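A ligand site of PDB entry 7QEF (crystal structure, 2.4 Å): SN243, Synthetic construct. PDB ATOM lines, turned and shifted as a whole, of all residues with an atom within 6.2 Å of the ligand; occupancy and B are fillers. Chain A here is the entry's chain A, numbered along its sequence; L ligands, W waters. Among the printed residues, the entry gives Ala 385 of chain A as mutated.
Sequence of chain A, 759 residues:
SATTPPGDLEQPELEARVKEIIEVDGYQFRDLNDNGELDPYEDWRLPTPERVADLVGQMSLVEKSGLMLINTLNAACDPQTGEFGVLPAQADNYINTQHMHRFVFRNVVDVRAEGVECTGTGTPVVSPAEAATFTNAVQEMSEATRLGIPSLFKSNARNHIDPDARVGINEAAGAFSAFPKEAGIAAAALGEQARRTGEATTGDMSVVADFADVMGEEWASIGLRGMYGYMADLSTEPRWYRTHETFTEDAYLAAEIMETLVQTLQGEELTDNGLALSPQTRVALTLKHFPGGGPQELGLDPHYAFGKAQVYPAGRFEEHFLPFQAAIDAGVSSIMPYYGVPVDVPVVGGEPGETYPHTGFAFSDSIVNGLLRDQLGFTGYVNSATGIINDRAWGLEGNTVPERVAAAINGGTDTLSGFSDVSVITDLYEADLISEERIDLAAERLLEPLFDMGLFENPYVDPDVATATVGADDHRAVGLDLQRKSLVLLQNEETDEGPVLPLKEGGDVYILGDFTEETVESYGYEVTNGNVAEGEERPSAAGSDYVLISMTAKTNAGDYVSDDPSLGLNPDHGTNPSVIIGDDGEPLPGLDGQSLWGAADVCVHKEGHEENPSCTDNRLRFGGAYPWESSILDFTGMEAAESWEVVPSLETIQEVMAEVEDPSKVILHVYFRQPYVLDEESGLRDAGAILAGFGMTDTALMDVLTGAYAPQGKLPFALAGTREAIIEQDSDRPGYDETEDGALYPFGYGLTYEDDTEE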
ATOM      1  N   THR A  72       7.194  14.463  11.720  1.00  0.00           N
ATOM      2  CA  THR A  72       8.024  13.288  11.994  1.00  0.00           C
ATOM      3  C   THR A  72       8.457  12.589  10.714  1.00  0.00           C
ATOM      4  O   THR A  72       7.622  12.182   9.890  1.00  0.00           O
ATOM      5  CB  THR A  72       7.278  12.289  12.882  1.00  0.00           C
ATOM      6  OG1 THR A  72       6.956  12.900  14.132  1.00  0.00           O
ATOM      7  CG2 THR A  72       8.126  11.073  13.114  1.00  0.00           C
ATOM      8  N   VAL A 104      11.151  16.124  11.905  1.00  0.00           N
ATOM      9  CA  VAL A 104      11.554  15.820  13.278  1.00  0.00           C
ATOM     10  C   VAL A 104      12.013  14.367  13.323  1.00  0.00           C
ATOM     11  O   VAL A 104      11.236  13.460  13.014  1.00  0.00           O
ATOM     12  CB  VAL A 104      10.414  16.068  14.269  1.00  0.00           C
ATOM     13  CG1 VAL A 104      10.903  15.876  15.687  1.00  0.00           C
ATOM     14  CG2 VAL A 104       9.878  17.481  14.071  1.00  0.00           C
ATOM     15  N   ARG A 106      13.244  11.182  15.381  1.00  0.00           N
ATOM     16  CA  ARG A 106      13.028  10.674  16.731  1.00  0.00           C
ATOM     17  C   ARG A 106      13.665   9.314  17.068  1.00  0.00           C
ATOM     18  O   ARG A 106      13.518   8.870  18.200  1.00  0.00           O
ATOM     19  CB  ARG A 106      11.510  10.584  17.012  1.00  0.00           C
ATOM     20  CG  ARG A 106      10.699  11.794  16.544  1.00  0.00           C
ATOM     21  CD  ARG A 106       9.215  11.655  16.929  1.00  0.00           C
ATOM     22  NE  ARG A 106       8.454  12.853  16.606  1.00  0.00           N
ATOM     23  CZ  ARG A 106       8.399  13.943  17.378  1.00  0.00           C
ATOM     24  NH1 ARG A 106       9.066  13.978  18.534  1.00  0.00           N
ATOM     25  NH2 ARG A 106       7.677  14.993  16.979  1.00  0.00           N
ATOM     26  N   ASN A 156      14.509  16.353  19.588  1.00  0.00           N
ATOM     27  CA  ASN A 156      14.622  16.688  21.001  1.00  0.00           C
ATOM     28  C   ASN A 156      16.024  16.321  21.495  1.00  0.00           C
ATOM     29  O   ASN A 156      16.804  15.699  20.773  1.00  0.00           O
ATOM     30  CB  ASN A 156      13.527  16.011  21.817  1.00  0.00           C
ATOM     31  CG  ASN A 156      12.126  16.528  21.446  1.00  0.00           C
ATOM     32  OD1 ASN A 156      11.785  17.697  21.703  1.00  0.00           O
ATOM     33  ND2 ASN A 156      11.337  15.657  20.822  1.00  0.00           N
ATOM     34  N   TYR A 228      14.517  20.839  18.588  1.00  0.00           N
ATOM     35  CA  TYR A 228      13.336  21.245  19.345  1.00  0.00           C
ATOM     36  C   TYR A 228      13.783  21.467  20.788  1.00  0.00           C
ATOM     37  O   TYR A 228      13.669  20.583  21.654  1.00  0.00           O
ATOM     38  CB  TYR A 228      12.239  20.192  19.253  1.00  0.00           C
ATOM     39  CG  TYR A 228      11.243  20.374  18.114  1.00  0.00           C
ATOM     40  CD1 TYR A 228      11.292  21.485  17.270  1.00  0.00           C
ATOM     41  CD2 TYR A 228      10.255  19.424  17.870  1.00  0.00           C
ATOM     42  CE1 TYR A 228      10.386  21.637  16.226  1.00  0.00           C
ATOM     43  CE2 TYR A 228       9.334  19.564  16.837  1.00  0.00           C
ATOM     44  CZ  TYR A 228       9.409  20.672  16.006  1.00  0.00           C
ATOM     45  OH  TYR A 228       8.509  20.815  14.978  1.00  0.00           O
ATOM     46  N   GLY A 229      14.312  22.660  21.039  1.00  0.00           N
ATOM     47  CA  GLY A 229      14.843  22.998  22.336  1.00  0.00           C
ATOM     48  C   GLY A 229      16.028  23.921  22.176  1.00  0.00           C
ATOM     49  O   GLY A 229      16.275  24.436  21.084  1.00  0.00           O
ATOM     50  N   MET A 231      14.974  23.929  26.466  1.00  0.00           N
ATOM     51  CA  MET A 231      13.877  24.549  27.207  1.00  0.00           C
ATOM     52  C   MET A 231      14.386  25.714  28.044  1.00  0.00           C
ATOM     53  O   MET A 231      15.295  25.560  28.855  1.00  0.00           O
ATOM     54  CB  MET A 231      13.197  23.515  28.098  1.00  0.00           C
ATOM     55  CG  MET A 231      12.173  22.740  27.302  1.00  0.00           C
ATOM     56  SD  MET A 231      11.553  21.250  28.053  1.00  0.00           S
ATOM     57  CE  MET A 231      10.751  21.915  29.548  1.00  0.00           C
ATOM     58  N   ARG A 242       7.247  18.301  33.598  1.00  0.00           N
ATOM     59  CA  ARG A 242       8.383  18.619  32.730  1.00  0.00           C
ATOM     60  C   ARG A 242       9.474  19.361  33.471  1.00  0.00           C
ATOM     61  O   ARG A 242      10.418  19.848  32.832  1.00  0.00           O
ATOM     62  CB  ARG A 242       7.953  19.449  31.514  1.00  0.00           C
ATOM     63  CG  ARG A 242       6.677  18.987  30.821  1.00  0.00           C
ATOM     64  CD  ARG A 242       6.511  19.574  29.402  1.00  0.00           C
ATOM     65  NE  ARG A 242       7.536  19.168  28.424  1.00  0.00           N
ATOM     66  CZ  ARG A 242       7.393  19.338  27.107  1.00  0.00           C
ATOM     67  NH1 ARG A 242       6.287  19.872  26.612  1.00  0.00           N
ATOM     68  NH2 ARG A 242       8.331  18.943  26.264  1.00  0.00           N
ATOM     69  N   GLU A 245      13.102  18.266  32.644  1.00  0.00           N
ATOM     70  CA  GLU A 245      13.979  18.745  31.589  1.00  0.00           C
ATOM     71  C   GLU A 245      14.167  20.267  31.648  1.00  0.00           C
ATOM     72  O   GLU A 245      14.632  20.862  30.679  1.00  0.00           O
ATOM     73  CB  GLU A 245      13.451  18.298  30.217  1.00  0.00           C
ATOM     74  CG  GLU A 245      11.949  18.420  30.019  1.00  0.00           C
ATOM     75  CD  GLU A 245      11.532  17.962  28.647  1.00  0.00           C
ATOM     76  OE1 GLU A 245      12.454  17.774  27.820  1.00  0.00           O
ATOM     77  OE2 GLU A 245      10.318  17.779  28.384  1.00  0.00           O
ATOM     78  N   LYS A 288      12.187  26.721  23.217  1.00  0.00           N
ATOM     79  CA  LYS A 288      10.852  26.381  23.625  1.00  0.00           C
ATOM     80  C   LYS A 288      10.792  26.527  25.151  1.00  0.00           C
ATOM     81  O   LYS A 288      11.829  26.583  25.818  1.00  0.00           O
ATOM     82  CB  LYS A 288      10.518  24.952  23.153  1.00  0.00           C
ATOM     83  CG  LYS A 288      11.402  23.880  23.771  1.00  0.00           C
ATOM     84  CD  LYS A 288      11.306  22.580  23.006  1.00  0.00           C
ATOM     85  CE  LYS A 288      11.600  21.418  23.936  1.00  0.00           C
ATOM     86  NZ  LYS A 288      11.530  20.168  23.178  1.00  0.00           N
ATOM     87  N   HIS A 289       9.578  26.671  25.684  1.00  0.00           N
ATOM     88  CA  HIS A 289       8.358  26.973  24.928  1.00  0.00           C
ATOM     89  C   HIS A 289       7.878  28.405  25.219  1.00  0.00           C
ATOM     90  O   HIS A 289       7.397  28.689  26.314  1.00  0.00           O
ATOM     91  CB  HIS A 289       7.262  25.976  25.268  1.00  0.00           C
ATOM     92  CG  HIS A 289       7.699  24.539  25.282  1.00  0.00           C
ATOM     93  ND1 HIS A 289       8.231  23.928  26.406  1.00  0.00           N
ATOM     94  CD2 HIS A 289       7.609  23.566  24.340  1.00  0.00           C
ATOM     95  CE1 HIS A 289       8.495  22.665  26.135  1.00  0.00           C
ATOM     96  NE2 HIS A 289       8.124  22.415  24.891  1.00  0.00           N
ATOM     97  N   HIS A 303      -0.488  19.865  27.361  1.00  0.00           N
ATOM     98  CA  HIS A 303      -0.717  18.787  26.398  1.00  0.00           C
ATOM     99  C   HIS A 303      -2.122  18.237  26.528  1.00  0.00           C
ATOM    100  O   HIS A 303      -2.655  17.641  25.580  1.00  0.00           O
ATOM    101  CB  HIS A 303       0.249  17.612  26.647  1.00  0.00           C
ATOM    102  CG  HIS A 303       1.574  17.686  25.955  1.00  0.00           C
ATOM    103  ND1 HIS A 303       2.708  18.207  26.565  1.00  0.00           N
ATOM    104  CD2 HIS A 303       1.998  17.181  24.766  1.00  0.00           C
ATOM    105  CE1 HIS A 303       3.743  18.073  25.751  1.00  0.00           C
ATOM    106  NE2 HIS A 303       3.344  17.450  24.653  1.00  0.00           N
ATOM    107  N   MET A 336       9.580  28.211  19.562  1.00  0.00           N
ATOM    108  CA  MET A 336       8.375  27.392  19.632  1.00  0.00           C
ATOM    109  C   MET A 336       7.512  27.902  20.769  1.00  0.00           C
ATOM    110  O   MET A 336       7.953  27.841  21.917  1.00  0.00           O
ATOM    111  CB  MET A 336       8.708  25.920  19.846  1.00  0.00           C
ATOM    112  CG  MET A 336       7.470  25.094  20.082  1.00  0.00           C
ATOM    113  SD  MET A 336       7.927  23.420  20.607  1.00  0.00           S
ATOM    114  CE  MET A 336       8.609  22.683  19.140  1.00  0.00           C
ATOM    115  N   TYR A 338       4.324  27.736  23.444  1.00  0.00           N
ATOM    116  CA  TYR A 338       3.697  26.611  24.142  1.00  0.00           C
ATOM    117  C   TYR A 338       2.191  26.563  23.885  1.00  0.00           C
ATOM    118  O   TYR A 338       1.575  27.527  23.433  1.00  0.00           O
ATOM    119  CB  TYR A 338       3.955  26.697  25.649  1.00  0.00           C
ATOM    120  CG  TYR A 338       3.997  25.325  26.308  1.00  0.00           C
ATOM    121  CD1 TYR A 338       4.420  24.218  25.584  1.00  0.00           C
ATOM    122  CD2 TYR A 338       3.603  25.139  27.645  1.00  0.00           C
ATOM    123  CE1 TYR A 338       4.471  22.964  26.162  1.00  0.00           C
ATOM    124  CE2 TYR A 338       3.658  23.884  28.245  1.00  0.00           C
ATOM    125  CZ  TYR A 338       4.096  22.784  27.496  1.00  0.00           C
ATOM    126  OH  TYR A 338       4.172  21.501  28.035  1.00  0.00           O
ATOM    127  N   TYR A 339       1.599  25.416  24.241  1.00  0.00           N
ATOM    128  CA  TYR A 339       0.159  25.204  24.107  1.00  0.00           C
ATOM    129  C   TYR A 339      -0.644  26.087  25.036  1.00  0.00           C
ATOM    130  O   TYR A 339      -1.807  26.367  24.756  1.00  0.00           O
ATOM    131  CB  TYR A 339      -0.195  23.752  24.417  1.00  0.00           C
ATOM    132  CG  TYR A 339       0.585  22.678  23.713  1.00  0.00           C
ATOM    133  CD1 TYR A 339       0.322  22.380  22.377  1.00  0.00           C
ATOM    134  CD2 TYR A 339       1.530  21.918  24.379  1.00  0.00           C
ATOM    135  CE1 TYR A 339       0.998  21.375  21.715  1.00  0.00           C
ATOM    136  CE2 TYR A 339       2.223  20.896  23.713  1.00  0.00           C
ATOM    137  CZ  TYR A 339       1.948  20.632  22.376  1.00  0.00           C
ATOM    138  OH  TYR A 339       2.579  19.650  21.684  1.00  0.00           O
ATOM    139  N   SER A 384       5.339  26.089  15.443  1.00  0.00           N
ATOM    140  CA  SER A 384       4.325  25.729  16.436  1.00  0.00           C
ATOM    141  C   SER A 384       4.750  24.498  17.240  1.00  0.00           C
ATOM    142  O   SER A 384       5.622  23.731  16.825  1.00  0.00           O
ATOM    143  CB  SER A 384       2.971  25.474  15.771  1.00  0.00           C
ATOM    144  OG  SER A 384       2.771  24.108  15.455  1.00  0.00           O
ATOM    145  N   ALA A 385       4.160  24.334  18.420  1.00  0.00           N
ATOM    146  CA  ALA A 385       4.292  23.059  19.113  1.00  0.00           C
ATOM    147  C   ALA A 385       3.481  22.006  18.368  1.00  0.00           C
ATOM    148  O   ALA A 385       2.515  22.306  17.650  1.00  0.00           O
ATOM    149  CB  ALA A 385       3.828  23.154  20.554  1.00  0.00           C
ATOM    150  N   THR A 386       3.830  20.745  18.602  1.00  0.00           N
ATOM    151  CA  THR A 386       3.281  19.677  17.788  1.00  0.00           C
ATOM    152  C   THR A 386       1.815  19.453  18.105  1.00  0.00           C
ATOM    153  O   THR A 386       1.400  19.464  19.284  1.00  0.00           O
ATOM    154  CB  THR A 386       4.112  18.403  17.992  1.00  0.00           C
ATOM    155  OG1 THR A 386       5.448  18.669  17.566  1.00  0.00           O
ATOM    156  CG2 THR A 386       3.552  17.202  17.226  1.00  0.00           C
ATOM    157  N   GLY A 387       0.995  19.379  17.043  1.00  0.00           N
ATOM    158  CA  GLY A 387      -0.392  18.988  17.161  1.00  0.00           C
ATOM    159  C   GLY A 387      -1.350  20.057  17.626  1.00  0.00           C
ATOM    160  O   GLY A 387      -2.420  19.723  18.156  1.00  0.00           O
ATOM    161  N   ASP A 391      -5.396  18.756  17.658  1.00  0.00           N
ATOM    162  CA  ASP A 391      -5.544  18.201  18.993  1.00  0.00           C
ATOM    163  C   ASP A 391      -5.557  19.239  20.095  1.00  0.00           C
ATOM    164  O   ASP A 391      -6.277  19.043  21.074  1.00  0.00           O
ATOM    165  CB  ASP A 391      -4.435  17.167  19.245  1.00  0.00           C
ATOM    166  CG  ASP A 391      -4.673  15.873  18.476  1.00  0.00           C
ATOM    167  OD1 ASP A 391      -5.849  15.477  18.380  1.00  0.00           O
ATOM    168  OD2 ASP A 391      -3.711  15.257  17.957  1.00  0.00           O
ATOM    169  N   ARG A 392      -4.752  20.300  19.998  1.00  0.00           N
ATOM    170  CA  ARG A 392      -4.598  21.234  21.112  1.00  0.00           C
ATOM    171  C   ARG A 392      -4.744  22.694  20.651  1.00  0.00           C
ATOM    172  O   ARG A 392      -3.952  23.577  21.002  1.00  0.00           O
ATOM    173  CB  ARG A 392      -3.265  20.980  21.817  1.00  0.00           C
ATOM    174  CG  ARG A 392      -3.054  19.499  22.169  1.00  0.00           C
ATOM    175  CD  ARG A 392      -1.744  19.143  22.908  1.00  0.00           C
ATOM    176  NE  ARG A 392      -1.639  17.681  22.934  1.00  0.00           N
ATOM    177  CZ  ARG A 392      -1.145  16.944  21.936  1.00  0.00           C
ATOM    178  NH1 ARG A 392      -0.676  17.527  20.838  1.00  0.00           N
ATOM    179  NH2 ARG A 392      -1.122  15.628  22.028  1.00  0.00           N
ATOM    180  N   SER A 417       4.112  22.226  13.312  1.00  0.00           N
ATOM    181  CA  SER A 417       4.527  20.890  13.720  1.00  0.00           C
ATOM    182  C   SER A 417       3.348  19.927  13.831  1.00  0.00           C
ATOM    183  O   SER A 417       2.424  20.158  14.610  1.00  0.00           O
ATOM    184  CB  SER A 417       5.272  20.939  15.049  1.00  0.00           C
ATOM    185  OG  SER A 417       5.832  19.672  15.310  1.00  0.00           O
ATOM    186  N   PHE A 622       2.271  11.731  27.592  1.00  0.00           N
ATOM    187  CA  PHE A 622       3.450  12.577  27.619  1.00  0.00           C
ATOM    188  C   PHE A 622       4.115  12.669  29.003  1.00  0.00           C
ATOM    189  O   PHE A 622       5.192  13.259  29.103  1.00  0.00           O
ATOM    190  CB  PHE A 622       3.055  13.949  27.091  1.00  0.00           C
ATOM    191  CG  PHE A 622       2.319  13.882  25.773  1.00  0.00           C
ATOM    192  CD1 PHE A 622       2.994  13.553  24.592  1.00  0.00           C
ATOM    193  CD2 PHE A 622       0.950  14.145  25.704  1.00  0.00           C
ATOM    194  CE1 PHE A 622       2.320  13.480  23.380  1.00  0.00           C
ATOM    195  CE2 PHE A 622       0.261  14.078  24.477  1.00  0.00           C
ATOM    196  CZ  PHE A 622       0.953  13.746  23.325  1.00  0.00           C
HETATM  197  C1  LIG L   1       7.517  17.368  19.698  1.00  0.00           C
HETATM  198  C2  LIG L   1       5.383  15.238  20.640  1.00  0.00           C
HETATM  199  C3  LIG L   1       3.233  14.652  19.788  1.00  0.00           C
HETATM  200  C4  LIG L   1       7.475  19.874  22.558  1.00  0.00           C
HETATM  201  C5  LIG L   1       6.239  19.179  23.075  1.00  0.00           C
HETATM  202  C6  LIG L   1       5.451  18.543  21.932  1.00  0.00           C
HETATM  203  C7  LIG L   1       7.273  18.732  20.359  1.00  0.00           C
HETATM  204  C8  LIG L   1       8.163  18.931  21.588  1.00  0.00           C
HETATM  205  C9  LIG L   1       4.810  16.328  21.265  1.00  0.00           C
HETATM  206  C10 LIG L   1       4.599  14.379  19.888  1.00  0.00           C
HETATM  207  C11 LIG L   1       2.649  15.729  20.446  1.00  0.00           C
HETATM  208  C12 LIG L   1       3.439  16.566  21.195  1.00  0.00           C
HETATM  209  N1  LIG L   1       2.411  13.762  18.996  1.00  0.00           N
HETATM  210  O1  LIG L   1       8.328  20.148  23.662  1.00  0.00           O
HETATM  211  O2  LIG L   1       5.381  19.977  23.891  1.00  0.00           O
HETATM  212  O3  LIG L   1       5.903  18.999  20.670  1.00  0.00           O
HETATM  213  O4  LIG L   1       9.438  19.438  21.165  1.00  0.00           O
HETATM  214  O5  LIG L   1       8.217  16.555  20.266  1.00  0.00           O
HETATM  215  O6  LIG L   1       7.050  17.130  18.605  1.00  0.00           O
HETATM  216  O7  LIG L   1       5.600  17.148  22.040  1.00  0.00           O
HETATM  217  O8  LIG L   1       2.915  12.737  18.544  1.00  0.00           O
HETATM  218  O9  LIG L   1       1.241  14.076  18.811  1.00  0.00           O
HETATM  219  O   HOH W   1       4.992  11.950  16.154  1.00  0.00           O
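The side-chain hydroxyl of Tyr 338 is in hydrogen-bond range of the guanidinium group of Arg 242 (3.0 Å).
OD1 of Asn 156 lies close to O of Tyr 228, at 3.4 Å.
The guanidinium group (NE) of Arg 392 is in hydrogen-bond range of the backbone carbonyl oxygen (O) of His 303 (2.8 Å).
The side-chain hydroxyl of Thr 386 sits at hydrogen-bond distance from the side-chain hydroxyl of Ser 417 (2.5 Å).
N of Arg 392 sits at hydrogen-bond distance from O of Gly 387 (3.0 Å).
The side-chain hydroxyl (OH) of Tyr 228 lies within hydrogen-bond range of the side-chain hydroxyl (OG) of Ser 417, at 2.9 Å.
O of Thr 386 is in hydrogen-bond range of OH of Tyr 339 (2.7 Å).
The guanidinium group (NE) of Arg 242 is in salt-bridge range of the side-chain carboxylate (OE2) of Glu 245.
Merely in contact with the ligand: Tyr 339 (3.1 Å), Tyr 228 (3.4 Å), Phe 622 (3.7 Å), Arg 392 (3.8 Å), Tyr 338 (3.9 Å) and Met 336 (3.9 Å).
Hydrophobic or aromatic side chains within 4 Å of the ligand: Tyr 228, His 289, His 303, Met 336, Tyr 338, Tyr 339 and Phe 622.
The guanidinium group of Arg 106 is in salt-bridge range of an oxygen (O6) of the ligand (2.8 Å).
The side-chain hydroxyl (OG1) of Thr 386 is in hydrogen-bond range of an oxygen (O6) of the ligand.
An oxygen (O4) of the ligand sits at hydrogen-bond distance from the side-chain amino group (NZ) of Lys 288, 3.0 Å away.
OD1 of Asn 156 sits at hydrogen-bond distance from O4 of the ligand (3.0 Å).
An oxygen (O3) of the ligand sits close to the backbone NH (N) of Thr 386, at 3.4 Å.
NH2 of Arg 242 lies within hydrogen-bond range of O1 of the ligand (2.9 Å).
An oxygen (O2) of the ligand lies close to a ring nitrogen (NE2) of His 303 (3.3 Å).
O1 of the ligand sits at hydrogen-bond distance from NE2 of His 289 (2.6 Å).
Water W1 lies within hydrogen-bond range of OG1 of Thr 72 (3.0 Å) and O8 of the ligand (3.3 Å).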
